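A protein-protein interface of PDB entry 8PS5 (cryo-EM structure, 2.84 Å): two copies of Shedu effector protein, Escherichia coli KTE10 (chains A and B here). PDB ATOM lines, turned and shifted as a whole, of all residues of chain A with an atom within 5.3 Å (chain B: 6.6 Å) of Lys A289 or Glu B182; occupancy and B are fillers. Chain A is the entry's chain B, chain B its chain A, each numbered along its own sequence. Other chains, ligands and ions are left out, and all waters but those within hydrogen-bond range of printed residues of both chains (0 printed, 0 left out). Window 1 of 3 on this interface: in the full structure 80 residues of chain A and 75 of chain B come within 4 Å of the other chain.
The backbone carbonyl oxygen of Leu A227 lies within hydrogen-bond range of the side-chain amino group of Lys A289 (3.1 Å). The guanidinium group (NH2) of Arg B178 lies within salt-bridge range of the side-chain carboxylate (OE2) of Glu B182, at 3.2 Å. O of Glu B182 is in hydrogen-bond range of ND2 of Asn B186, 3.0 Å away.
The side-chain carboxylate of Glu B182 sits close to the side-chain carboxylate of Glu A229 (2.9 Å). The guanidinium group (NH1) of Arg B178 lies within salt-bridge range of the side-chain carboxylate (OE2) of Glu A310 (3.7 Å). OE1 of Glu B182 is in salt-bridge range of NZ of Lys A289, 2.8 Å away.
Of chain B, only Glu B182 (2.8 Å) and Leu B185 (3.7 Å) come within 4 Å of Lys A289. Printed residues of chain B within 4 Å of Phe A291: Ala B161 (3.6 Å), Arg B178 (3.5 Å), Tyr B181 (3.7 Å) and Glu B182 (3.7 Å). Of the printed residues of chain B, Asn A226 touches Leu B185. Printed residues of chain B within 4 Å of Ser A228: Leu B185 (3.4 Å) and Asn B186 (3.6 Å). Of the printed residues of chain B, Glu A229 touches Glu B182 (2.9 Å) and Asn B186 (3.7 Å). Printed residues of chain A within 4 Å of Tyr B181: Phe A291. Glu B179 touches none of the printed residues of chain A. Val A361 touches none of the printed residues of chain B. The nearest residue of chain B that does not touch Lys A289 is Tyr B181 (4.2 Å). The nearest printed residue of chain A that does not touch Asn B186 is Leu A227 (7.0 Å).
Of the 15 printed residues of chain A, 6 touch a printed residue of chain B. Hydrophobic or aromatic side chains of chain A that line the printed part of chain B: Phe A291. Printed residues of chain B that touch a printed residue of chain A: Ala B161, Arg B178, Tyr B181, Glu B182, Leu B185 and Asn B186. Along chain B the printed residues that touch a printed residue of chain A span positions 161 to 186. Among the printed residues, 12 pairs touch across the chains. Among the printed residues, Asp or Glu carboxylates within 4 Å of a Lys or Arg side-chain nitrogen of the other chain: Lys A289 with Glu B182 and Glu A310 with Arg B178.
No position is printed for both chains. Of the 12 pairs that touch across the chains among the printed residues, none has its exchanged pair printed and touching as well.
Among the printed residues, pairs that only touch across the chains: Ser A228 with Leu B185, Phe A291 with Arg B178, Ser A228 with Asn B186, Phe A291 with Ala B161, Lys A289 with Leu B185, Phe A291 with Glu B182, Glu A229 with Asn B186, Phe A291 with Tyr B181 and Asn A226 with Leu B185.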
ATOM      1  N   THR A 225      14.202  -4.430 -24.779  1.00  0.00           N
ATOM      2  CA  THR A 225      14.290  -5.235 -23.563  1.00  0.00           C
ATOM      3  C   THR A 225      13.031  -6.080 -23.376  1.00  0.00           C
ATOM      4  O   THR A 225      13.101  -7.230 -22.923  1.00  0.00           O
ATOM      5  CB  THR A 225      14.535  -4.311 -22.363  1.00  0.00           C
ATOM      6  OG1 THR A 225      15.706  -3.522 -22.609  1.00  0.00           O
ATOM      7  CG2 THR A 225      14.765  -5.092 -21.073  1.00  0.00           C
ATOM      8  N   ASN A 226      11.877  -5.562 -23.811  1.00  0.00           N
ATOM      9  CA  ASN A 226      10.594  -6.200 -23.527  1.00  0.00           C
ATOM     10  C   ASN A 226      10.285  -7.382 -24.444  1.00  0.00           C
ATOM     11  O   ASN A 226       9.225  -7.998 -24.293  1.00  0.00           O
ATOM     12  CB  ASN A 226       9.472  -5.167 -23.624  1.00  0.00           C
ATOM     13  CG  ASN A 226       9.721  -4.138 -24.708  1.00  0.00           C
ATOM     14  OD1 ASN A 226       9.773  -4.468 -25.891  1.00  0.00           O
ATOM     15  ND2 ASN A 226       9.883  -2.884 -24.307  1.00  0.00           N
ATOM     16  N   LEU A 227      11.168  -7.708 -25.383  1.00  0.00           N
ATOM     17  CA  LEU A 227      10.989  -8.858 -26.257  1.00  0.00           C
ATOM     18  C   LEU A 227      11.260 -10.159 -25.499  1.00  0.00           C
ATOM     19  O   LEU A 227      11.782 -10.164 -24.384  1.00  0.00           O
ATOM     20  CB  LEU A 227      11.921  -8.748 -27.464  1.00  0.00           C
ATOM     21  CG  LEU A 227      11.757  -7.556 -28.417  1.00  0.00           C
ATOM     22  CD1 LEU A 227      12.485  -7.797 -29.725  1.00  0.00           C
ATOM     23  CD2 LEU A 227      10.293  -7.246 -28.690  1.00  0.00           C
ATOM     24  N   SER A 228      10.907 -11.278 -26.130  1.00  0.00           N
ATOM     25  CA  SER A 228      11.185 -12.591 -25.563  1.00  0.00           C
ATOM     26  C   SER A 228      12.653 -12.970 -25.795  1.00  0.00           C
ATOM     27  O   SER A 228      13.401 -12.258 -26.464  1.00  0.00           O
ATOM     28  CB  SER A 228      10.246 -13.632 -26.167  1.00  0.00           C
ATOM     29  OG  SER A 228      10.684 -14.039 -27.450  1.00  0.00           O
ATOM     30  N   GLU A 229      13.071 -14.110 -25.227  1.00  0.00           N
ATOM     31  CA  GLU A 229      14.468 -14.515 -25.381  1.00  0.00           C
ATOM     32  C   GLU A 229      14.731 -15.092 -26.757  1.00  0.00           C
ATOM     33  O   GLU A 229      15.881 -15.148 -27.193  1.00  0.00           O
ATOM     34  CB  GLU A 229      14.892 -15.558 -24.357  1.00  0.00           C
ATOM     35  CG  GLU A 229      14.847 -15.156 -22.941  1.00  0.00           C
ATOM     36  CD  GLU A 229      13.606 -15.678 -22.322  1.00  0.00           C
ATOM     37  OE1 GLU A 229      12.507 -15.265 -22.727  1.00  0.00           O
ATOM     38  OE2 GLU A 229      13.737 -16.577 -21.483  1.00  0.00           O
ATOM     39  N   TRP A 232      15.283 -11.845 -28.525  1.00  0.00           N
ATOM     40  CA  TRP A 232      16.544 -11.263 -28.060  1.00  0.00           C
ATOM     41  C   TRP A 232      17.747 -12.054 -28.562  1.00  0.00           C
ATOM     42  O   TRP A 232      18.763 -11.472 -28.968  1.00  0.00           O
ATOM     43  CB  TRP A 232      16.554 -11.199 -26.533  1.00  0.00           C
ATOM     44  CG  TRP A 232      17.794 -10.596 -25.963  1.00  0.00           C
ATOM     45  CD1 TRP A 232      18.885 -11.258 -25.481  1.00  0.00           C
ATOM     46  CD2 TRP A 232      18.068  -9.203 -25.804  1.00  0.00           C
ATOM     47  NE1 TRP A 232      19.825 -10.362 -25.041  1.00  0.00           N
ATOM     48  CE2 TRP A 232      19.347  -9.093 -25.226  1.00  0.00           C
ATOM     49  CE3 TRP A 232      17.358  -8.037 -26.098  1.00  0.00           C
ATOM     50  CZ2 TRP A 232      19.929  -7.863 -24.938  1.00  0.00           C
ATOM     51  CZ3 TRP A 232      17.936  -6.823 -25.810  1.00  0.00           C
ATOM     52  CH2 TRP A 232      19.209  -6.742 -25.235  1.00  0.00           C
ATOM     53  N   VAL A 287      23.044 -16.512 -23.906  1.00  0.00           N
ATOM     54  CA  VAL A 287      22.664 -15.115 -24.070  1.00  0.00           C
ATOM     55  C   VAL A 287      21.305 -14.946 -23.409  1.00  0.00           C
ATOM     56  O   VAL A 287      20.284 -15.409 -23.935  1.00  0.00           O
ATOM     57  CB  VAL A 287      22.634 -14.697 -25.548  1.00  0.00           C
ATOM     58  CG1 VAL A 287      22.133 -13.268 -25.697  1.00  0.00           C
ATOM     59  CG2 VAL A 287      24.013 -14.836 -26.157  1.00  0.00           C
ATOM     60  N   LYS A 288      21.296 -14.310 -22.244  1.00  0.00           N
ATOM     61  CA  LYS A 288      20.102 -14.165 -21.427  1.00  0.00           C
ATOM     62  C   LYS A 288      19.548 -12.762 -21.600  1.00  0.00           C
ATOM     63  O   LYS A 288      20.314 -11.799 -21.705  1.00  0.00           O
ATOM     64  CB  LYS A 288      20.411 -14.442 -19.954  1.00  0.00           C
ATOM     65  CG  LYS A 288      21.010 -15.814 -19.688  1.00  0.00           C
ATOM     66  CD  LYS A 288      19.926 -16.867 -19.540  1.00  0.00           C
ATOM     67  CE  LYS A 288      19.982 -17.887 -20.662  1.00  0.00           C
ATOM     68  NZ  LYS A 288      18.668 -18.552 -20.871  1.00  0.00           N
ATOM     69  N   LYS A 289      18.226 -12.654 -21.654  1.00  0.00           N
ATOM     70  CA  LYS A 289      17.588 -11.358 -21.806  1.00  0.00           C
ATOM     71  C   LYS A 289      17.673 -10.583 -20.490  1.00  0.00           C
ATOM     72  O   LYS A 289      17.426 -11.152 -19.419  1.00  0.00           O
ATOM     73  CB  LYS A 289      16.135 -11.545 -22.257  1.00  0.00           C
ATOM     74  CG  LYS A 289      15.115 -10.555 -21.725  1.00  0.00           C
ATOM     75  CD  LYS A 289      13.720 -11.126 -21.860  1.00  0.00           C
ATOM     76  CE  LYS A 289      12.697 -10.303 -21.107  1.00  0.00           C
ATOM     77  NZ  LYS A 289      11.316 -10.782 -21.381  1.00  0.00           N
ATOM     78  N   PRO A 290      18.056  -9.297 -20.524  1.00  0.00           N
ATOM     79  CA  PRO A 290      18.266  -8.539 -19.270  1.00  0.00           C
ATOM     80  C   PRO A 290      16.961  -8.087 -18.624  1.00  0.00           C
ATOM     81  O   PRO A 290      16.496  -6.951 -18.762  1.00  0.00           O
ATOM     82  CB  PRO A 290      19.139  -7.370 -19.737  1.00  0.00           C
ATOM     83  CG  PRO A 290      18.779  -7.165 -21.162  1.00  0.00           C
ATOM     84  CD  PRO A 290      18.343  -8.486 -21.720  1.00  0.00           C
ATOM     85  N   PHE A 291      16.341  -9.010 -17.886  1.00  0.00           N
ATOM     86  CA  PHE A 291      15.103  -8.691 -17.182  1.00  0.00           C
ATOM     87  C   PHE A 291      15.367  -7.850 -15.939  1.00  0.00           C
ATOM     88  O   PHE A 291      14.589  -6.945 -15.618  1.00  0.00           O
ATOM     89  CB  PHE A 291      14.370  -9.979 -16.813  1.00  0.00           C
ATOM     90  CG  PHE A 291      12.943  -9.767 -16.408  1.00  0.00           C
ATOM     91  CD1 PHE A 291      11.973  -9.488 -17.362  1.00  0.00           C
ATOM     92  CD2 PHE A 291      12.571  -9.846 -15.073  1.00  0.00           C
ATOM     93  CE1 PHE A 291      10.653  -9.292 -16.990  1.00  0.00           C
ATOM     94  CE2 PHE A 291      11.255  -9.651 -14.693  1.00  0.00           C
ATOM     95  CZ  PHE A 291      10.295  -9.373 -15.653  1.00  0.00           C
ATOM     96  N   ASP A 292      16.456  -8.129 -15.230  1.00  0.00           N
ATOM     97  CA  ASP A 292      16.794  -7.439 -13.995  1.00  0.00           C
ATOM     98  C   ASP A 292      17.972  -6.501 -14.219  1.00  0.00           C
ATOM     99  O   ASP A 292      18.823  -6.738 -15.081  1.00  0.00           O
ATOM    100  CB  ASP A 292      17.127  -8.435 -12.881  1.00  0.00           C
ATOM    101  CG  ASP A 292      16.863  -7.873 -11.501  1.00  0.00           C
ATOM    102  OD1 ASP A 292      16.220  -6.807 -11.404  1.00  0.00           O
ATOM    103  OD2 ASP A 292      17.297  -8.499 -10.513  1.00  0.00           O
ATOM    104  N   GLU A 310      19.395 -15.179 -11.123  1.00  0.00           N
ATOM    105  CA  GLU A 310      19.442 -15.171 -12.586  1.00  0.00           C
ATOM    106  C   GLU A 310      20.796 -15.645 -13.098  1.00  0.00           C
ATOM    107  O   GLU A 310      20.875 -16.488 -14.007  1.00  0.00           O
ATOM    108  CB  GLU A 310      19.147 -13.762 -13.101  1.00  0.00           C
ATOM    109  CG  GLU A 310      18.634 -13.695 -14.528  1.00  0.00           C
ATOM    110  CD  GLU A 310      18.663 -12.284 -15.090  1.00  0.00           C
ATOM    111  OE1 GLU A 310      19.052 -11.355 -14.352  1.00  0.00           O
ATOM    112  OE2 GLU A 310      18.302 -12.104 -16.272  1.00  0.00           O
ATOM    113  N   VAL A 361      24.353 -12.080 -19.129  1.00  0.00           N
ATOM    114  CA  VAL A 361      23.126 -12.220 -18.345  1.00  0.00           C
ATOM    115  C   VAL A 361      22.366 -10.900 -18.264  1.00  0.00           C
ATOM    116  O   VAL A 361      21.243 -10.783 -18.768  1.00  0.00           O
ATOM    117  CB  VAL A 361      23.431 -12.776 -16.940  1.00  0.00           C
ATOM    118  CG1 VAL A 361      24.309 -11.806 -16.168  1.00  0.00           C
ATOM    119  CG2 VAL A 361      22.159 -13.080 -16.157  1.00  0.00           C
ATOM    120  N   TYR A 395      25.923  -7.113 -19.952  1.00  0.00           N
ATOM    121  CA  TYR A 395      25.828  -6.382 -21.207  1.00  0.00           C
ATOM    122  C   TYR A 395      26.671  -5.119 -21.153  1.00  0.00           C
ATOM    123  O   TYR A 395      27.225  -4.683 -22.170  1.00  0.00           O
ATOM    124  CB  TYR A 395      24.370  -6.085 -21.528  1.00  0.00           C
ATOM    125  CG  TYR A 395      23.666  -7.312 -22.043  1.00  0.00           C
ATOM    126  CD1 TYR A 395      23.801  -7.705 -23.372  1.00  0.00           C
ATOM    127  CD2 TYR A 395      22.896  -8.096 -21.193  1.00  0.00           C
ATOM    128  CE1 TYR A 395      23.171  -8.843 -23.845  1.00  0.00           C
ATOM    129  CE2 TYR A 395      22.262  -9.231 -21.655  1.00  0.00           C
ATOM    130  CZ  TYR A 395      22.402  -9.598 -22.980  1.00  0.00           C
ATOM    131  OH  TYR A 395      21.770 -10.726 -23.442  1.00  0.00           O
ATOM    132  N   ARG B 157       1.519 -12.738 -15.301  1.00  0.00           N
ATOM    133  CA  ARG B 157       2.789 -13.454 -15.350  1.00  0.00           C
ATOM    134  C   ARG B 157       3.971 -12.494 -15.321  1.00  0.00           C
ATOM    135  O   ARG B 157       4.995 -12.789 -14.694  1.00  0.00           O
ATOM    136  CB  ARG B 157       2.837 -14.334 -16.598  1.00  0.00           C
ATOM    137  CG  ARG B 157       2.695 -15.813 -16.304  1.00  0.00           C
ATOM    138  CD  ARG B 157       2.464 -16.610 -17.569  1.00  0.00           C
ATOM    139  NE  ARG B 157       1.184 -16.296 -18.191  1.00  0.00           N
ATOM    140  CZ  ARG B 157       0.091 -17.035 -18.065  1.00  0.00           C
ATOM    141  NH1 ARG B 157       0.083 -18.138 -17.338  1.00  0.00           N
ATOM    142  NH2 ARG B 157      -1.021 -16.657 -18.686  1.00  0.00           N
ATOM    143  N   ALA B 161       6.620 -12.320 -12.328  1.00  0.00           N
ATOM    144  CA  ALA B 161       8.032 -12.413 -12.685  1.00  0.00           C
ATOM    145  C   ALA B 161       8.825 -11.215 -12.179  1.00  0.00           C
ATOM    146  O   ALA B 161       9.995 -11.355 -11.806  1.00  0.00           O
ATOM    147  CB  ALA B 161       8.181 -12.545 -14.199  1.00  0.00           C
ATOM    148  N   ALA B 177       8.176 -18.019 -11.291  1.00  0.00           N
ATOM    149  CA  ALA B 177       7.317 -17.173 -12.110  1.00  0.00           C
ATOM    150  C   ALA B 177       8.060 -16.643 -13.325  1.00  0.00           C
ATOM    151  O   ALA B 177       7.439 -16.315 -14.344  1.00  0.00           O
ATOM    152  CB  ALA B 177       6.776 -16.018 -11.276  1.00  0.00           C
ATOM    153  N   ARG B 178       9.387 -16.532 -13.225  1.00  0.00           N
ATOM    154  CA  ARG B 178      10.193 -16.090 -14.358  1.00  0.00           C
ATOM    155  C   ARG B 178      10.219 -17.140 -15.457  1.00  0.00           C
ATOM    156  O   ARG B 178      10.153 -16.798 -16.642  1.00  0.00           O
ATOM    157  CB  ARG B 178      11.610 -15.757 -13.892  1.00  0.00           C
ATOM    158  CG  ARG B 178      11.706 -14.441 -13.143  1.00  0.00           C
ATOM    159  CD  ARG B 178      12.809 -13.538 -13.671  1.00  0.00           C
ATOM    160  NE  ARG B 178      12.818 -13.429 -15.124  1.00  0.00           N
ATOM    161  CZ  ARG B 178      13.916 -13.480 -15.866  1.00  0.00           C
ATOM    162  NH1 ARG B 178      15.114 -13.613 -15.320  1.00  0.00           N
ATOM    163  NH2 ARG B 178      13.811 -13.380 -17.188  1.00  0.00           N
ATOM    164  N   GLU B 179      10.270 -18.423 -15.075  1.00  0.00           N
ATOM    165  CA  GLU B 179      10.218 -19.520 -16.040  1.00  0.00           C
ATOM    166  C   GLU B 179       8.872 -19.570 -16.748  1.00  0.00           C
ATOM    167  O   GLU B 179       8.815 -19.716 -17.974  1.00  0.00           O
ATOM    168  CB  GLU B 179      10.511 -20.846 -15.334  1.00  0.00           C
ATOM    169  CG  GLU B 179      10.194 -22.098 -16.139  1.00  0.00           C
ATOM    170  CD  GLU B 179      11.000 -22.195 -17.413  1.00  0.00           C
ATOM    171  OE1 GLU B 179      12.241 -22.133 -17.338  1.00  0.00           O
ATOM    172  OE2 GLU B 179      10.394 -22.352 -18.491  1.00  0.00           O
ATOM    173  N   ARG B 180       7.785 -19.349 -16.001  1.00  0.00           N
ATOM    174  CA  ARG B 180       6.447 -19.367 -16.587  1.00  0.00           C
ATOM    175  C   ARG B 180       6.202 -18.159 -17.486  1.00  0.00           C
ATOM    176  O   ARG B 180       5.617 -18.298 -18.567  1.00  0.00           O
ATOM    177  CB  ARG B 180       5.393 -19.438 -15.484  1.00  0.00           C
ATOM    178  CG  ARG B 180       4.077 -20.039 -15.945  1.00  0.00           C
ATOM    179  CD  ARG B 180       3.166 -20.361 -14.777  1.00  0.00           C
ATOM    180  NE  ARG B 180       2.509 -19.172 -14.256  1.00  0.00           N
ATOM    181  CZ  ARG B 180       1.196 -18.984 -14.245  1.00  0.00           C
ATOM    182  NH1 ARG B 180       0.364 -19.899 -14.715  1.00  0.00           N
ATOM    183  NH2 ARG B 180       0.707 -17.851 -13.749  1.00  0.00           N
ATOM    184  N   TYR B 181       6.691 -16.978 -17.088  1.00  0.00           N
ATOM    185  CA  TYR B 181       6.475 -15.778 -17.896  1.00  0.00           C
ATOM    186  C   TYR B 181       7.331 -15.787 -19.158  1.00  0.00           C
ATOM    187  O   TYR B 181       6.855 -15.425 -20.241  1.00  0.00           O
ATOM    188  CB  TYR B 181       6.749 -14.521 -17.072  1.00  0.00           C
ATOM    189  CG  TYR B 181       6.849 -13.257 -17.903  1.00  0.00           C
ATOM    190  CD1 TYR B 181       5.757 -12.782 -18.634  1.00  0.00           C
ATOM    191  CD2 TYR B 181       8.037 -12.540 -17.954  1.00  0.00           C
ATOM    192  CE1 TYR B 181       5.857 -11.630 -19.396  1.00  0.00           C
ATOM    193  CE2 TYR B 181       8.146 -11.388 -18.711  1.00  0.00           C
ATOM    194  CZ  TYR B 181       7.054 -10.940 -19.426  1.00  0.00           C
ATOM    195  OH  TYR B 181       7.168  -9.795 -20.176  1.00  0.00           O
ATOM    196  N   GLU B 182       8.598 -16.202 -19.049  1.00  0.00           N
ATOM    197  CA  GLU B 182       9.440 -16.245 -20.239  1.00  0.00           C
ATOM    198  C   GLU B 182       9.096 -17.434 -21.131  1.00  0.00           C
ATOM    199  O   GLU B 182       9.380 -17.408 -22.334  1.00  0.00           O
ATOM    200  CB  GLU B 182      10.918 -16.282 -19.859  1.00  0.00           C
ATOM    201  CG  GLU B 182      11.520 -15.094 -19.073  1.00  0.00           C
ATOM    202  CD  GLU B 182      11.242 -13.699 -19.626  1.00  0.00           C
ATOM    203  OE1 GLU B 182      11.186 -13.500 -20.855  1.00  0.00           O
ATOM    204  OE2 GLU B 182      11.130 -12.769 -18.805  1.00  0.00           O
ATOM    205  N   HIS B 183       8.487 -18.486 -20.575  1.00  0.00           N
ATOM    206  CA  HIS B 183       7.991 -19.564 -21.421  1.00  0.00           C
ATOM    207  C   HIS B 183       6.700 -19.156 -22.116  1.00  0.00           C
ATOM    208  O   HIS B 183       6.416 -19.609 -23.230  1.00  0.00           O
ATOM    209  CB  HIS B 183       7.784 -20.830 -20.591  1.00  0.00           C
ATOM    210  CG  HIS B 183       7.466 -22.043 -21.409  1.00  0.00           C
ATOM    211  ND1 HIS B 183       6.181 -22.374 -21.783  1.00  0.00           N
ATOM    212  CD2 HIS B 183       8.267 -23.002 -21.929  1.00  0.00           C
ATOM    213  CE1 HIS B 183       6.205 -23.484 -22.497  1.00  0.00           C
ATOM    214  NE2 HIS B 183       7.458 -23.887 -22.601  1.00  0.00           N
ATOM    215  N   TYR B 184       5.901 -18.306 -21.466  1.00  0.00           N
ATOM    216  CA  TYR B 184       4.695 -17.781 -22.095  1.00  0.00           C
ATOM    217  C   TYR B 184       5.035 -16.776 -23.187  1.00  0.00           C
ATOM    218  O   TYR B 184       4.322 -16.668 -24.190  1.00  0.00           O
ATOM    219  CB  TYR B 184       3.799 -17.149 -21.030  1.00  0.00           C
ATOM    220  CG  TYR B 184       2.533 -16.520 -21.562  1.00  0.00           C
ATOM    221  CD1 TYR B 184       1.441 -17.306 -21.912  1.00  0.00           C
ATOM    222  CD2 TYR B 184       2.420 -15.137 -21.690  1.00  0.00           C
ATOM    223  CE1 TYR B 184       0.277 -16.734 -22.395  1.00  0.00           C
ATOM    224  CE2 TYR B 184       1.264 -14.560 -22.176  1.00  0.00           C
ATOM    225  CZ  TYR B 184       0.197 -15.362 -22.521  1.00  0.00           C
ATOM    226  OH  TYR B 184      -0.956 -14.785 -22.999  1.00  0.00           O
ATOM    227  N   LEU B 185       6.120 -16.020 -23.004  1.00  0.00           N
ATOM    228  CA  LEU B 185       6.463 -14.981 -23.971  1.00  0.00           C
ATOM    229  C   LEU B 185       7.112 -15.566 -25.220  1.00  0.00           C
ATOM    230  O   LEU B 185       7.146 -14.913 -26.271  1.00  0.00           O
ATOM    231  CB  LEU B 185       7.381 -13.948 -23.322  1.00  0.00           C
ATOM    232  CG  LEU B 185       7.156 -12.495 -23.734  1.00  0.00           C
ATOM    233  CD1 LEU B 185       5.734 -12.078 -23.433  1.00  0.00           C
ATOM    234  CD2 LEU B 185       8.138 -11.591 -23.020  1.00  0.00           C
ATOM    235  N   ASN B 186       7.618 -16.799 -25.133  1.00  0.00           N
ATOM    236  CA  ASN B 186       8.334 -17.397 -26.256  1.00  0.00           C
ATOM    237  C   ASN B 186       7.383 -17.859 -27.354  1.00  0.00           C
ATOM    238  O   ASN B 186       7.798 -18.049 -28.503  1.00  0.00           O
ATOM    239  CB  ASN B 186       9.190 -18.566 -25.769  1.00  0.00           C
ATOM    240  CG  ASN B 186      10.565 -18.131 -25.317  1.00  0.00           C
ATOM    241  OD1 ASN B 186      11.131 -17.182 -25.852  1.00  0.00           O
ATOM    242  ND2 ASN B 186      11.109 -18.825 -24.328  1.00  0.00           N
ATOM    243  N   ARG B 187       6.103 -18.048 -27.025  1.00  0.00           N
ATOM    244  CA  ARG B 187       5.142 -18.464 -28.041  1.00  0.00           C
ATOM    245  C   ARG B 187       4.576 -17.264 -28.791  1.00  0.00           C
ATOM    246  O   ARG B 187       3.881 -17.424 -29.800  1.00  0.00           O
ATOM    247  CB  ARG B 187       4.020 -19.279 -27.402  1.00  0.00           C
ATOM    248  CG  ARG B 187       2.972 -18.451 -26.683  1.00  0.00           C
ATOM    249  CD  ARG B 187       1.811 -19.298 -26.163  1.00  0.00           C
ATOM    250  NE  ARG B 187       2.111 -19.950 -24.892  1.00  0.00           N
ATOM    251  CZ  ARG B 187       2.551 -21.195 -24.761  1.00  0.00           C
ATOM    252  NH1 ARG B 187       2.714 -21.987 -25.808  1.00  0.00           N
ATOM    253  NH2 ARG B 187       2.821 -21.662 -23.546  1.00  0.00           N
